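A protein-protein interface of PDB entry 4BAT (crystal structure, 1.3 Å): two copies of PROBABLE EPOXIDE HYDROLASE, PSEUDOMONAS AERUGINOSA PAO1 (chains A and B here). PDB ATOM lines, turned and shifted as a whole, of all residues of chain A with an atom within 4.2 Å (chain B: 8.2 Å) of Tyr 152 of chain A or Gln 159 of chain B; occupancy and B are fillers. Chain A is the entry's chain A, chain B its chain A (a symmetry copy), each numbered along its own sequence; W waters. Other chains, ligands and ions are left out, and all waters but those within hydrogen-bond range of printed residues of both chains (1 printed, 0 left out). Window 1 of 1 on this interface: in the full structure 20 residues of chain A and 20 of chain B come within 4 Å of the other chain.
O of Leu 149 of chain A sits at hydrogen-bond distance from NE2 of Gln 159 of chain B. The guanidinium group (NH1) of Arg 182 of chain A lies within hydrogen-bond range of the side-chain amide oxygen (OE1) of Gln 159 of chain B, at 2.8 Å.
The backbone carbonyl oxygen of Leu 149 of chain A lies within hydrogen-bond range of the guanidinium group of Arg 182 of chain A (3.3 Å). The guanidinium group of Arg 182 of chain A is in hydrogen-bond range of the backbone carbonyl oxygen of Asn 150 of chain A. The backbone carbonyl oxygen (O) of Phe 155 of chain B lies within hydrogen-bond range of the side-chain amide nitrogen (NE2) of Gln 159 of chain B, 2.9 Å away. O of Gln 159 of chain B is in hydrogen-bond range of NH2 of Arg 216 of chain B (2.9 Å).
Ala 148 of chain A touches Ala 148 of chain B (CB to CB, 3.9 Å). CB of Ala 148 of chain A touches CD1 of Phe 155 of chain B, at 3.5 Å. N of Leu 149 of chain A touches CD1 of Phe 155 of chain B, at 3.8 Å. Leu 149 of chain A touches Ala 158 of chain B (CD2 to CB, 3.97 Å). CG1 of Val 219 of chain B touches CD1 of Leu 149 of chain A, 3.6 Å away. Tyr 152 of chain A touches Leu 156 of chain B. Tyr 152 of chain A touches Gln 159 of chain B (CB to NE2, 3.5 Å). CD1 of Leu 163 of chain B touches OH of Tyr 152 of chain A (3.8 Å). Phe 155 of chain A touches Leu 149 of chain B (CD1 to N, 3.8 Å). Leu 156 of chain A touches Tyr 152 of chain B.
No residue of chain B comes within 4 Å of Ala 151 of chain A. Of chain B, only Leu 156, Gln 159 and Leu 163 come within 4 Å of Tyr 152 of chain A. Of the printed residues of chain A, Ala 148 of chain B touches Ala 148 and Phe 155. Of the printed residues of chain A, Tyr 152 of chain B touches Leu 156. Printed residues of chain A within 4 Å of Phe 155 of chain B: Ala 148 and Leu 149. Of the printed residues of chain A, Ala 158 of chain B touches Leu 149. Arg 216 of chain B touches none of the printed residues of chain A. Of the printed residues of chain A, Val 219 of chain B touches Leu 149. The nearest residue of chain B that does not touch Tyr 152 of chain A is Phe 155 of chain B (4.05 Å). The nearest printed residue of chain B that does not touch Leu 156 of chain A is Leu 167 of chain B (4.2 Å).
Printed residues of chain B that touch a printed residue of chain A: Ala 148, Leu 149, Tyr 152, Phe 155, Leu 156, Ala 158, Gln 159, Leu 163 and Val 219. Hydrophobic or aromatic side chains of chain B that line the printed part of chain A: Ala 148, Leu 149, Tyr 152, Phe 155, Leu 156, Ala 158, Leu 163 and Val 219. Hydrophobic or aromatic side chains of chain A that line the printed part of chain B: Ala 148, Leu 149, Tyr 152, Phe 155 and Leu 156. Among the printed residues, 13 pairs touch across the chains. Among the printed residues, no Asp or Glu carboxylate lies within 4 Å of a Lys or Arg side-chain nitrogen of the other chain.
Ala 148 of chain A touches its own counterpart, Ala 148 of chain B. Ala 148 of chain A touches Phe 155 of chain B, and with the chains exchanged Phe 155 of chain A touches Ala 148 of chain B. Leu 149 of chain A touches Phe 155 of chain B, and with the chains exchanged Phe 155 of chain A touches Leu 149 of chain B. Tyr 152 of chain A touches Leu 156 of chain B, and with the chains exchanged Leu 156 of chain A touches Tyr 152 of chain B. Positions printed for both chains: 148, 149, 152, 153, 154, 155 and 156. Of the 13 pairs that touch across the chains among the printed residues, 7 have their exchanged pair printed and touching as well.
Water W1 bridges O of Tyr 152 of chain A (2.9 Å) and O of Tyr 152 of chain B (2.9 Å).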
ATOM      1  N   ALA A 148     -11.816  19.339 -11.459  1.00  0.00           N
ATOM      2  CA  ALA A 148     -12.532  18.654 -12.530  1.00  0.00           C
ATOM      3  C   ALA A 148     -13.836  19.358 -12.896  1.00  0.00           C
ATOM      4  O   ALA A 148     -14.269  19.320 -14.061  1.00  0.00           O
ATOM      5  CB  ALA A 148     -12.729  17.173 -12.210  1.00  0.00           C
ATOM      6  N   LEU A 149     -14.482  20.012 -11.943  1.00  0.00           N
ATOM      7  CA  LEU A 149     -15.666  20.831 -12.259  1.00  0.00           C
ATOM      8  C   LEU A 149     -15.291  22.070 -13.046  1.00  0.00           C
ATOM      9  O   LEU A 149     -15.975  22.455 -13.995  1.00  0.00           O
ATOM     10  CB  LEU A 149     -16.439  21.160 -10.986  1.00  0.00           C
ATOM     11  CG  LEU A 149     -17.161  19.962 -10.339  1.00  0.00           C
ATOM     12  CD1 LEU A 149     -17.596  20.273  -8.918  1.00  0.00           C
ATOM     13  CD2 LEU A 149     -18.376  19.533 -11.193  1.00  0.00           C
ATOM     14  N   ASN A 150     -14.258  22.761 -12.582  1.00  0.00           N
ATOM     15  CA  ASN A 150     -13.815  24.016 -13.196  1.00  0.00           C
ATOM     16  C   ASN A 150     -13.357  23.738 -14.643  1.00  0.00           C
ATOM     17  O   ASN A 150     -13.729  24.468 -15.570  1.00  0.00           O
ATOM     18  CB  ASN A 150     -12.667  24.646 -12.352  1.00  0.00           C
ATOM     19  CG  ASN A 150     -13.180  25.359 -11.092  1.00  0.00           C
ATOM     20  OD1 ASN A 150     -14.370  25.450 -10.899  1.00  0.00           O
ATOM     21  ND2 ASN A 150     -12.268  25.856 -10.232  1.00  0.00           N
ATOM     22  N   ALA A 151     -12.514  22.708 -14.789  1.00  0.00           N
ATOM     23  CA  ALA A 151     -11.858  22.336 -16.051  1.00  0.00           C
ATOM     24  C   ALA A 151     -12.488  21.065 -16.632  1.00  0.00           C
ATOM     25  O   ALA A 151     -11.785  20.180 -17.136  1.00  0.00           O
ATOM     26  CB  ALA A 151     -10.363  22.179 -15.887  1.00  0.00           C
ATOM     27  N   TYR A 152     -13.821  20.983 -16.610  1.00  0.00           N
ATOM     28  CA  TYR A 152     -14.514  19.784 -17.073  1.00  0.00           C
ATOM     29  C   TYR A 152     -14.127  19.431 -18.501  1.00  0.00           C
ATOM     30  O   TYR A 152     -14.132  18.233 -18.854  1.00  0.00           O
ATOM     31  CB  TYR A 152     -16.046  19.928 -16.931  1.00  0.00           C
ATOM     32  CG  TYR A 152     -16.644  20.708 -18.073  1.00  0.00           C
ATOM     33  CD1 TYR A 152     -16.557  22.098 -18.113  1.00  0.00           C
ATOM     34  CD2 TYR A 152     -17.172  20.048 -19.168  1.00  0.00           C
ATOM     35  CE1 TYR A 152     -16.963  22.834 -19.235  1.00  0.00           C
ATOM     36  CE2 TYR A 152     -17.611  20.754 -20.297  1.00  0.00           C
ATOM     37  CZ  TYR A 152     -17.483  22.150 -20.322  1.00  0.00           C
ATOM     38  OH  TYR A 152     -17.887  22.802 -21.484  1.00  0.00           O
ATOM     39  N   HIS A 153     -13.820  20.444 -19.320  1.00  0.00           N
ATOM     40  CA  HIS A 153     -13.511  20.207 -20.711  1.00  0.00           C
ATOM     41  C   HIS A 153     -12.206  19.463 -20.892  1.00  0.00           C
ATOM     42  O   HIS A 153     -11.999  18.815 -21.919  1.00  0.00           O
ATOM     43  CB  HIS A 153     -13.544  21.517 -21.504  1.00  0.00           C
ATOM     44  CG  HIS A 153     -12.508  22.458 -21.091  1.00  0.00           C
ATOM     45  ND1 HIS A 153     -12.511  23.040 -19.834  1.00  0.00           N
ATOM     46  CD2 HIS A 153     -11.400  22.932 -21.757  1.00  0.00           C
ATOM     47  CE1 HIS A 153     -11.474  23.856 -19.739  1.00  0.00           C
ATOM     48  NE2 HIS A 153     -10.786  23.817 -20.905  1.00  0.00           N
ATOM     49  N   TRP A 154     -11.303  19.532 -19.933  1.00  0.00           N
ATOM     50  CA  TRP A 154     -10.061  18.763 -20.026  1.00  0.00           C
ATOM     51  C   TRP A 154     -10.347  17.264 -20.064  1.00  0.00           C
ATOM     52  O   TRP A 154      -9.592  16.487 -20.649  1.00  0.00           O
ATOM     53  CB  TRP A 154      -9.149  19.032 -18.821  1.00  0.00           C
ATOM     54  CG  TRP A 154      -8.467  20.348 -18.890  1.00  0.00           C
ATOM     55  CD1 TRP A 154      -8.942  21.532 -19.385  1.00  0.00           C
ATOM     56  CD2 TRP A 154      -7.145  20.627 -18.376  1.00  0.00           C
ATOM     57  NE1 TRP A 154      -7.996  22.531 -19.263  1.00  0.00           N
ATOM     58  CE2 TRP A 154      -6.882  22.024 -18.676  1.00  0.00           C
ATOM     59  CE3 TRP A 154      -6.162  19.849 -17.760  1.00  0.00           C
ATOM     60  CZ2 TRP A 154      -5.672  22.626 -18.310  1.00  0.00           C
ATOM     61  CZ3 TRP A 154      -4.957  20.453 -17.450  1.00  0.00           C
ATOM     62  CH2 TRP A 154      -4.719  21.804 -17.753  1.00  0.00           C
ATOM     63  N   PHE A 155     -11.449  16.872 -19.425  1.00  0.00           N
ATOM     64  CA  PHE A 155     -11.871  15.490 -19.345  1.00  0.00           C
ATOM     65  C   PHE A 155     -12.813  15.123 -20.479  1.00  0.00           C
ATOM     66  O   PHE A 155     -12.671  14.056 -21.054  1.00  0.00           O
ATOM     67  CB  PHE A 155     -12.440  15.231 -17.949  1.00  0.00           C
ATOM     68  CG  PHE A 155     -11.425  15.580 -16.886  1.00  0.00           C
ATOM     69  CD1 PHE A 155     -10.383  14.718 -16.618  1.00  0.00           C
ATOM     70  CD2 PHE A 155     -11.460  16.791 -16.268  1.00  0.00           C
ATOM     71  CE1 PHE A 155      -9.363  15.069 -15.745  1.00  0.00           C
ATOM     72  CE2 PHE A 155     -10.462  17.175 -15.389  1.00  0.00           C
ATOM     73  CZ  PHE A 155      -9.425  16.312 -15.120  1.00  0.00           C
ATOM     74  N   LEU A 156     -13.700  16.053 -20.850  1.00  0.00           N
ATOM     75  CA  LEU A 156     -14.595  15.791 -21.984  1.00  0.00           C
ATOM     76  C   LEU A 156     -13.800  15.619 -23.283  1.00  0.00           C
ATOM     77  O   LEU A 156     -14.007  14.681 -24.064  1.00  0.00           O
ATOM     78  CB  LEU A 156     -15.632  16.934 -22.148  1.00  0.00           C
ATOM     79  CG  LEU A 156     -16.488  16.896 -23.418  1.00  0.00           C
ATOM     80  CD1 LEU A 156     -17.340  15.634 -23.530  1.00  0.00           C
ATOM     81  CD2 LEU A 156     -17.319  18.186 -23.493  1.00  0.00           C
ATOM     82  N   PHE A 175     -21.065  26.508 -28.471  1.00  0.00           N
ATOM     83  CA  PHE A 175     -20.043  25.993 -27.564  1.00  0.00           C
ATOM     84  C   PHE A 175     -18.827  26.919 -27.515  1.00  0.00           C
ATOM     85  O   PHE A 175     -18.289  27.198 -26.431  1.00  0.00           O
ATOM     86  CB  PHE A 175     -19.616  24.568 -27.942  1.00  0.00           C
ATOM     87  CG  PHE A 175     -18.636  23.982 -26.979  1.00  0.00           C
ATOM     88  CD1 PHE A 175     -19.094  23.477 -25.800  1.00  0.00           C
ATOM     89  CD2 PHE A 175     -17.293  23.970 -27.231  1.00  0.00           C
ATOM     90  CE1 PHE A 175     -18.208  22.977 -24.868  1.00  0.00           C
ATOM     91  CE2 PHE A 175     -16.398  23.443 -26.315  1.00  0.00           C
ATOM     92  CZ  PHE A 175     -16.873  22.928 -25.136  1.00  0.00           C
ATOM     93  N   ARG A 182     -16.758  32.056 -20.610  1.00  0.00           N
ATOM     94  CA  ARG A 182     -16.356  31.440 -19.364  1.00  0.00           C
ATOM     95  C   ARG A 182     -14.874  31.655 -19.062  1.00  0.00           C
ATOM     96  O   ARG A 182     -14.493  31.997 -17.948  1.00  0.00           O
ATOM     97  CB  ARG A 182     -16.698  29.950 -19.419  1.00  0.00           C
ATOM     98  CG  ARG A 182     -16.321  29.183 -18.186  1.00  0.00           C
ATOM     99  CD  ARG A 182     -17.011  27.866 -18.155  1.00  0.00           C
ATOM    100  NE  ARG A 182     -16.483  27.000 -17.103  1.00  0.00           N
ATOM    101  CZ  ARG A 182     -17.074  25.907 -16.673  1.00  0.00           C
ATOM    102  NH1 ARG A 182     -18.293  25.600 -17.087  1.00  0.00           N
ATOM    103  NH2 ARG A 182     -16.493  25.173 -15.726  1.00  0.00           N
ATOM    104  N   ALA B 148     -11.615  11.257 -13.028  1.00  0.00           N
ATOM    105  CA  ALA B 148     -12.286  12.273 -13.834  1.00  0.00           C
ATOM    106  C   ALA B 148     -12.344  11.892 -15.310  1.00  0.00           C
ATOM    107  O   ALA B 148     -13.295  12.260 -16.020  1.00  0.00           O
ATOM    108  CB  ALA B 148     -11.681  13.657 -13.602  1.00  0.00           C
ATOM    109  N   LEU B 149     -11.359  11.158 -15.805  1.00  0.00           N
ATOM    110  CA  LEU B 149     -11.426  10.636 -17.183  1.00  0.00           C
ATOM    111  C   LEU B 149     -12.482   9.559 -17.319  1.00  0.00           C
ATOM    112  O   LEU B 149     -13.224   9.514 -18.301  1.00  0.00           O
ATOM    113  CB  LEU B 149     -10.049  10.164 -17.638  1.00  0.00           C
ATOM    114  CG  LEU B 149      -9.023  11.290 -17.874  1.00  0.00           C
ATOM    115  CD1 LEU B 149      -7.608  10.746 -17.969  1.00  0.00           C
ATOM    116  CD2 LEU B 149      -9.379  12.092 -19.147  1.00  0.00           C
ATOM    117  N   TYR B 152     -16.096  11.157 -16.657  1.00  0.00           N
ATOM    118  CA  TYR B 152     -16.119  12.527 -17.163  1.00  0.00           C
ATOM    119  C   TYR B 152     -17.518  13.120 -17.106  1.00  0.00           C
ATOM    120  O   TYR B 152     -17.650  14.351 -16.938  1.00  0.00           O
ATOM    121  CB  TYR B 152     -15.538  12.609 -18.593  1.00  0.00           C
ATOM    122  CG  TYR B 152     -16.552  12.212 -19.634  1.00  0.00           C
ATOM    123  CD1 TYR B 152     -16.845  10.871 -19.873  1.00  0.00           C
ATOM    124  CD2 TYR B 152     -17.307  13.178 -20.276  1.00  0.00           C
ATOM    125  CE1 TYR B 152     -17.893  10.481 -20.719  1.00  0.00           C
ATOM    126  CE2 TYR B 152     -18.347  12.823 -21.148  1.00  0.00           C
ATOM    127  CZ  TYR B 152     -18.639  11.467 -21.346  1.00  0.00           C
ATOM    128  OH  TYR B 152     -19.711  11.165 -22.182  1.00  0.00           O
ATOM    129  N   HIS B 153     -18.547  12.279 -17.264  1.00  0.00           N
ATOM    130  CA  HIS B 153     -19.906  12.766 -17.295  1.00  0.00           C
ATOM    131  C   HIS B 153     -20.355  13.307 -15.955  1.00  0.00           C
ATOM    132  O   HIS B 153     -21.275  14.124 -15.893  1.00  0.00           O
ATOM    133  CB  HIS B 153     -20.855  11.690 -17.831  1.00  0.00           C
ATOM    134  CG  HIS B 153     -20.942  10.522 -16.959  1.00  0.00           C
ATOM    135  ND1 HIS B 153     -19.859   9.683 -16.754  1.00  0.00           N
ATOM    136  CD2 HIS B 153     -21.985  10.033 -16.205  1.00  0.00           C
ATOM    137  CE1 HIS B 153     -20.223   8.707 -15.939  1.00  0.00           C
ATOM    138  NE2 HIS B 153     -21.521   8.891 -15.599  1.00  0.00           N
ATOM    139  N   TRP B 154     -19.745  12.878 -14.867  1.00  0.00           N
ATOM    140  CA  TRP B 154     -20.088  13.432 -13.556  1.00  0.00           C
ATOM    141  C   TRP B 154     -19.790  14.929 -13.500  1.00  0.00           C
ATOM    142  O   TRP B 154     -20.442  15.680 -12.777  1.00  0.00           O
ATOM    143  CB  TRP B 154     -19.284  12.755 -12.438  1.00  0.00           C
ATOM    144  CG  TRP B 154     -19.776  11.394 -12.111  1.00  0.00           C
ATOM    145  CD1 TRP B 154     -20.289  10.445 -12.953  1.00  0.00           C
ATOM    146  CD2 TRP B 154     -19.747  10.793 -10.796  1.00  0.00           C
ATOM    147  NE1 TRP B 154     -20.630   9.302 -12.257  1.00  0.00           N
ATOM    148  CE2 TRP B 154     -20.339   9.475 -10.941  1.00  0.00           C
ATOM    149  CE3 TRP B 154     -19.344  11.242  -9.536  1.00  0.00           C
ATOM    150  CZ2 TRP B 154     -20.468   8.615  -9.844  1.00  0.00           C
ATOM    151  CZ3 TRP B 154     -19.524  10.394  -8.458  1.00  0.00           C
ATOM    152  CH2 TRP B 154     -20.104   9.124  -8.618  1.00  0.00           C
ATOM    153  N   PHE B 155     -18.787  15.344 -14.274  1.00  0.00           N
ATOM    154  CA  PHE B 155     -18.355  16.723 -14.340  1.00  0.00           C
ATOM    155  C   PHE B 155     -19.067  17.484 -15.445  1.00  0.00           C
ATOM    156  O   PHE B 155     -19.474  18.614 -15.228  1.00  0.00           O
ATOM    157  CB  PHE B 155     -16.829  16.755 -14.440  1.00  0.00           C
ATOM    158  CG  PHE B 155     -16.202  16.015 -13.282  1.00  0.00           C
ATOM    159  CD1 PHE B 155     -16.129  16.612 -12.041  1.00  0.00           C
ATOM    160  CD2 PHE B 155     -15.812  14.720 -13.417  1.00  0.00           C
ATOM    161  CE1 PHE B 155     -15.684  15.912 -10.928  1.00  0.00           C
ATOM    162  CE2 PHE B 155     -15.358  13.990 -12.332  1.00  0.00           C
ATOM    163  CZ  PHE B 155     -15.284  14.589 -11.096  1.00  0.00           C
ATOM    164  N   LEU B 156     -19.294  16.820 -16.584  1.00  0.00           N
ATOM    165  CA  LEU B 156     -20.039  17.471 -17.668  1.00  0.00           C
ATOM    166  C   LEU B 156     -21.471  17.795 -17.234  1.00  0.00           C
ATOM    167  O   LEU B 156     -21.986  18.904 -17.429  1.00  0.00           O
ATOM    168  CB  LEU B 156     -20.060  16.581 -18.939  1.00  0.00           C
ATOM    169  CG  LEU B 156     -20.981  17.041 -20.073  1.00  0.00           C
ATOM    170  CD1 LEU B 156     -20.616  18.419 -20.621  1.00  0.00           C
ATOM    171  CD2 LEU B 156     -21.008  15.955 -21.160  1.00  0.00           C
ATOM    172  N   LEU B 157     -22.182  16.784 -16.748  1.00  0.00           N
ATOM    173  CA  LEU B 157     -23.617  16.904 -16.479  1.00  0.00           C
ATOM    174  C   LEU B 157     -23.901  17.827 -15.295  1.00  0.00           C
ATOM    175  O   LEU B 157     -25.021  18.353 -15.180  1.00  0.00           O
ATOM    176  CB  LEU B 157     -24.259  15.537 -16.259  1.00  0.00           C
ATOM    177  CG  LEU B 157     -24.128  14.529 -17.390  1.00  0.00           C
ATOM    178  CD1 LEU B 157     -24.683  13.180 -16.983  1.00  0.00           C
ATOM    179  CD2 LEU B 157     -24.767  15.074 -18.664  1.00  0.00           C
ATOM    180  N   ALA B 158     -22.881  18.131 -14.469  1.00  0.00           N
ATOM    181  CA  ALA B 158     -22.996  19.055 -13.357  1.00  0.00           C
ATOM    182  C   ALA B 158     -22.687  20.493 -13.716  1.00  0.00           C
ATOM    183  O   ALA B 158     -22.835  21.352 -12.847  1.00  0.00           O
ATOM    184  CB  ALA B 158     -22.108  18.609 -12.199  1.00  0.00           C
ATOM    185  N   GLN B 159     -22.316  20.767 -14.957  1.00  0.00           N
ATOM    186  CA  GLN B 159     -22.055  22.164 -15.336  1.00  0.00           C
ATOM    187  C   GLN B 159     -23.365  22.960 -15.315  1.00  0.00           C
ATOM    188  O   GLN B 159     -24.456  22.374 -15.405  1.00  0.00           O
ATOM    189  CB  GLN B 159     -21.386  22.250 -16.703  1.00  0.00           C
ATOM    190  CG  GLN B 159     -20.029  21.570 -16.701  1.00  0.00           C
ATOM    191  CD  GLN B 159     -19.091  22.150 -15.675  1.00  0.00           C
ATOM    192  OE1 GLN B 159     -18.920  23.363 -15.611  1.00  0.00           O
ATOM    193  NE2 GLN B 159     -18.496  21.280 -14.859  1.00  0.00           N
ATOM    194  N   PRO B 160     -23.287  24.292 -15.183  1.00  0.00           N
ATOM    195  CA  PRO B 160     -24.516  25.065 -15.048  1.00  0.00           C
ATOM    196  C   PRO B 160     -25.448  24.942 -16.232  1.00  0.00           C
ATOM    197  O   PRO B 160     -25.034  24.771 -17.380  1.00  0.00           O
ATOM    198  CB  PRO B 160     -24.029  26.481 -14.889  1.00  0.00           C
ATOM    199  CG  PRO B 160     -22.647  26.322 -14.329  1.00  0.00           C
ATOM    200  CD  PRO B 160     -22.083  25.103 -14.977  1.00  0.00           C
ATOM    201  N   TYR B 161     -26.731  25.053 -15.936  1.00  0.00           N
ATOM    202  CA  TYR B 161     -27.774  25.077 -16.945  1.00  0.00           C
ATOM    203  C   TYR B 161     -27.456  26.161 -17.970  1.00  0.00           C
ATOM    204  O   TYR B 161     -27.113  27.284 -17.557  1.00  0.00           O
ATOM    205  CB  TYR B 161     -29.114  25.390 -16.274  1.00  0.00           C
ATOM    206  CG  TYR B 161     -30.255  25.396 -17.236  1.00  0.00           C
ATOM    207  CD1 TYR B 161     -30.799  24.223 -17.740  1.00  0.00           C
ATOM    208  CD2 TYR B 161     -30.800  26.598 -17.659  1.00  0.00           C
ATOM    209  CE1 TYR B 161     -31.841  24.250 -18.624  1.00  0.00           C
ATOM    210  CE2 TYR B 161     -31.842  26.636 -18.568  1.00  0.00           C
ATOM    211  CZ  TYR B 161     -32.375  25.466 -19.048  1.00  0.00           C
ATOM    212  OH  TYR B 161     -33.428  25.482 -19.930  1.00  0.00           O
ATOM    213  N   ASP B 162     -27.546  25.906 -19.271  1.00  0.00           N
ATOM    214  CA  ASP B 162     -28.020  24.707 -19.984  1.00  0.00           C
ATOM    215  C   ASP B 162     -26.915  24.057 -20.799  1.00  0.00           C
ATOM    216  O   ASP B 162     -27.155  23.481 -21.843  1.00  0.00           O
ATOM    217  CB  ASP B 162     -29.203  25.069 -20.883  1.00  0.00           C
ATOM    218  CG  ASP B 162     -28.853  26.032 -22.011  1.00  0.00           C
ATOM    219  OD1 ASP B 162     -27.818  26.723 -21.945  1.00  0.00           O
ATOM    220  OD2 ASP B 162     -29.712  26.162 -22.911  1.00  0.00           O
ATOM    221  N   LEU B 163     -25.659  24.157 -20.310  1.00  0.00           N
ATOM    222  CA  LEU B 163     -24.516  23.658 -21.054  1.00  0.00           C
ATOM    223  C   LEU B 163     -24.651  22.151 -21.402  1.00  0.00           C
ATOM    224  O   LEU B 163     -24.646  21.773 -22.582  1.00  0.00           O
ATOM    225  CB  LEU B 163     -23.193  24.025 -20.393  1.00  0.00           C
ATOM    226  CG  LEU B 163     -21.900  23.557 -21.077  1.00  0.00           C
ATOM    227  CD1 LEU B 163     -21.540  22.102 -20.892  1.00  0.00           C
ATOM    228  CD2 LEU B 163     -21.789  24.026 -22.511  1.00  0.00           C
ATOM    229  N   PRO B 164     -24.774  21.289 -20.387  1.00  0.00           N
ATOM    230  CA  PRO B 164     -24.825  19.896 -20.757  1.00  0.00           C
ATOM    231  C   PRO B 164     -26.122  19.514 -21.482  1.00  0.00           C
ATOM    232  O   PRO B 164     -26.104  18.651 -22.402  1.00  0.00           O
ATOM    233  CB  PRO B 164     -24.724  19.130 -19.439  1.00  0.00           C
ATOM    234  CG  PRO B 164     -25.209  20.115 -18.404  1.00  0.00           C
ATOM    235  CD  PRO B 164     -24.741  21.471 -18.927  1.00  0.00           C
ATOM    236  N   GLU B 165     -27.238  20.191 -21.150  1.00  0.00           N
ATOM    237  CA  GLU B 165     -28.482  19.931 -21.869  1.00  0.00           C
ATOM    238  C   GLU B 165     -28.307  20.189 -23.372  1.00  0.00           C
ATOM    239  O   GLU B 165     -28.771  19.411 -24.216  1.00  0.00           O
ATOM    240  CB  GLU B 165     -29.646  20.769 -21.342  1.00  0.00           C
ATOM    241  CG  GLU B 165     -30.170  20.388 -19.967  1.00  0.00           C
ATOM    242  CD  GLU B 165     -29.467  20.989 -18.765  1.00  0.00           C
ATOM    243  OE1 GLU B 165     -28.347  21.547 -18.902  1.00  0.00           O
ATOM    244  OE2 GLU B 165     -30.030  20.885 -17.663  1.00  0.00           O
ATOM    245  N   LEU B 167     -25.495  20.039 -25.109  1.00  0.00           N
ATOM    246  CA  LEU B 167     -24.575  19.058 -25.711  1.00  0.00           C
ATOM    247  C   LEU B 167     -25.225  17.671 -25.852  1.00  0.00           C
ATOM    248  O   LEU B 167     -25.132  17.051 -26.913  1.00  0.00           O
ATOM    249  CB  LEU B 167     -23.274  18.988 -24.927  1.00  0.00           C
ATOM    250  CG  LEU B 167     -22.411  20.243 -24.903  1.00  0.00           C
ATOM    251  CD1 LEU B 167     -21.080  19.946 -24.212  1.00  0.00           C
ATOM    252  CD2 LEU B 167     -22.161  20.800 -26.267  1.00  0.00           C
ATOM    253  N   CYS B 212     -29.415  15.928 -15.620  1.00  0.00           N
ATOM    254  CA  CYS B 212     -28.422  16.958 -15.302  1.00  0.00           C
ATOM    255  C   CYS B 212     -28.642  17.452 -13.890  1.00  0.00           C
ATOM    256  O   CYS B 212     -27.679  17.698 -13.161  1.00  0.00           O
ATOM    257  CB  CYS B 212     -28.374  18.079 -16.346  1.00  0.00           C
ATOM    258  SG  CYS B 212     -27.876  17.544 -17.996  1.00  0.00           S
ATOM    259  N   GLU B 213     -29.901  17.753 -13.536  1.00  0.00           N
ATOM    260  CA  GLU B 213     -30.183  18.211 -12.199  1.00  0.00           C
ATOM    261  C   GLU B 213     -29.727  17.222 -11.107  1.00  0.00           C
ATOM    262  O   GLU B 213     -29.225  17.696 -10.070  1.00  0.00           O
ATOM    263  CB  GLU B 213     -31.639  18.556 -12.035  1.00  0.00           C
ATOM    264  CG  GLU B 213     -32.075  19.788 -12.786  1.00  0.00           C
ATOM    265  CD  GLU B 213     -31.501  21.061 -12.203  1.00  0.00           C
ATOM    266  OE1 GLU B 213     -31.800  21.393 -11.017  1.00  0.00           O
ATOM    267  OE2 GLU B 213     -30.698  21.748 -12.869  1.00  0.00           O
ATOM    268  N   TYR B 215     -27.123  15.166 -11.347  1.00  0.00           N
ATOM    269  CA  TYR B 215     -25.684  15.315 -11.274  1.00  0.00           C
ATOM    270  C   TYR B 215     -25.262  16.650 -10.609  1.00  0.00           C
ATOM    271  O   TYR B 215     -24.234  16.684  -9.910  1.00  0.00           O
ATOM    272  CB  TYR B 215     -25.060  15.100 -12.654  1.00  0.00           C
ATOM    273  CG  TYR B 215     -24.984  13.618 -13.011  1.00  0.00           C
ATOM    274  CD1 TYR B 215     -26.021  12.925 -13.588  1.00  0.00           C
ATOM    275  CD2 TYR B 215     -23.882  12.901 -12.668  1.00  0.00           C
ATOM    276  CE1 TYR B 215     -25.932  11.576 -13.853  1.00  0.00           C
ATOM    277  CE2 TYR B 215     -23.785  11.555 -12.952  1.00  0.00           C
ATOM    278  CZ  TYR B 215     -24.825  10.887 -13.522  1.00  0.00           C
ATOM    279  OH  TYR B 215     -24.735   9.532 -13.814  1.00  0.00           O
ATOM    280  N   ARG B 216     -26.018  17.743 -10.834  1.00  0.00           N
ATOM    281  CA  ARG B 216     -25.765  19.006 -10.124  1.00  0.00           C
ATOM    282  C   ARG B 216     -25.972  18.852  -8.611  1.00  0.00           C
ATOM    283  O   ARG B 216     -25.180  19.358  -7.801  1.00  0.00           O
ATOM    284  CB  ARG B 216     -26.656  20.112 -10.681  1.00  0.00           C
ATOM    285  CG  ARG B 216     -26.342  20.541 -12.102  1.00  0.00           C
ATOM    286  CD  ARG B 216     -27.352  21.523 -12.690  1.00  0.00           C
ATOM    287  NE  ARG B 216     -26.966  21.851 -14.035  1.00  0.00           N
ATOM    288  CZ  ARG B 216     -27.690  21.645 -15.141  1.00  0.00           C
ATOM    289  NH1 ARG B 216     -28.969  21.359 -15.078  1.00  0.00           N
ATOM    290  NH2 ARG B 216     -27.102  21.758 -16.307  1.00  0.00           N
ATOM    291  N   VAL B 219     -23.057  17.132  -6.765  1.00  0.00           N
ATOM    292  CA  VAL B 219     -21.969  18.049  -6.444  1.00  0.00           C
ATOM    293  C   VAL B 219     -22.270  18.869  -5.211  1.00  0.00           C
ATOM    294  O   VAL B 219     -21.394  19.108  -4.369  1.00  0.00           O
ATOM    295  CB  VAL B 219     -21.645  18.947  -7.669  1.00  0.00           C
ATOM    296  CG1 VAL B 219     -20.794  20.149  -7.294  1.00  0.00           C
ATOM    297  CG2 VAL B 219     -20.996  18.123  -8.769  1.00  0.00           C
HETATM  298  O   HOH W   1     -16.443  16.424 -18.643  1.00  0.00           O
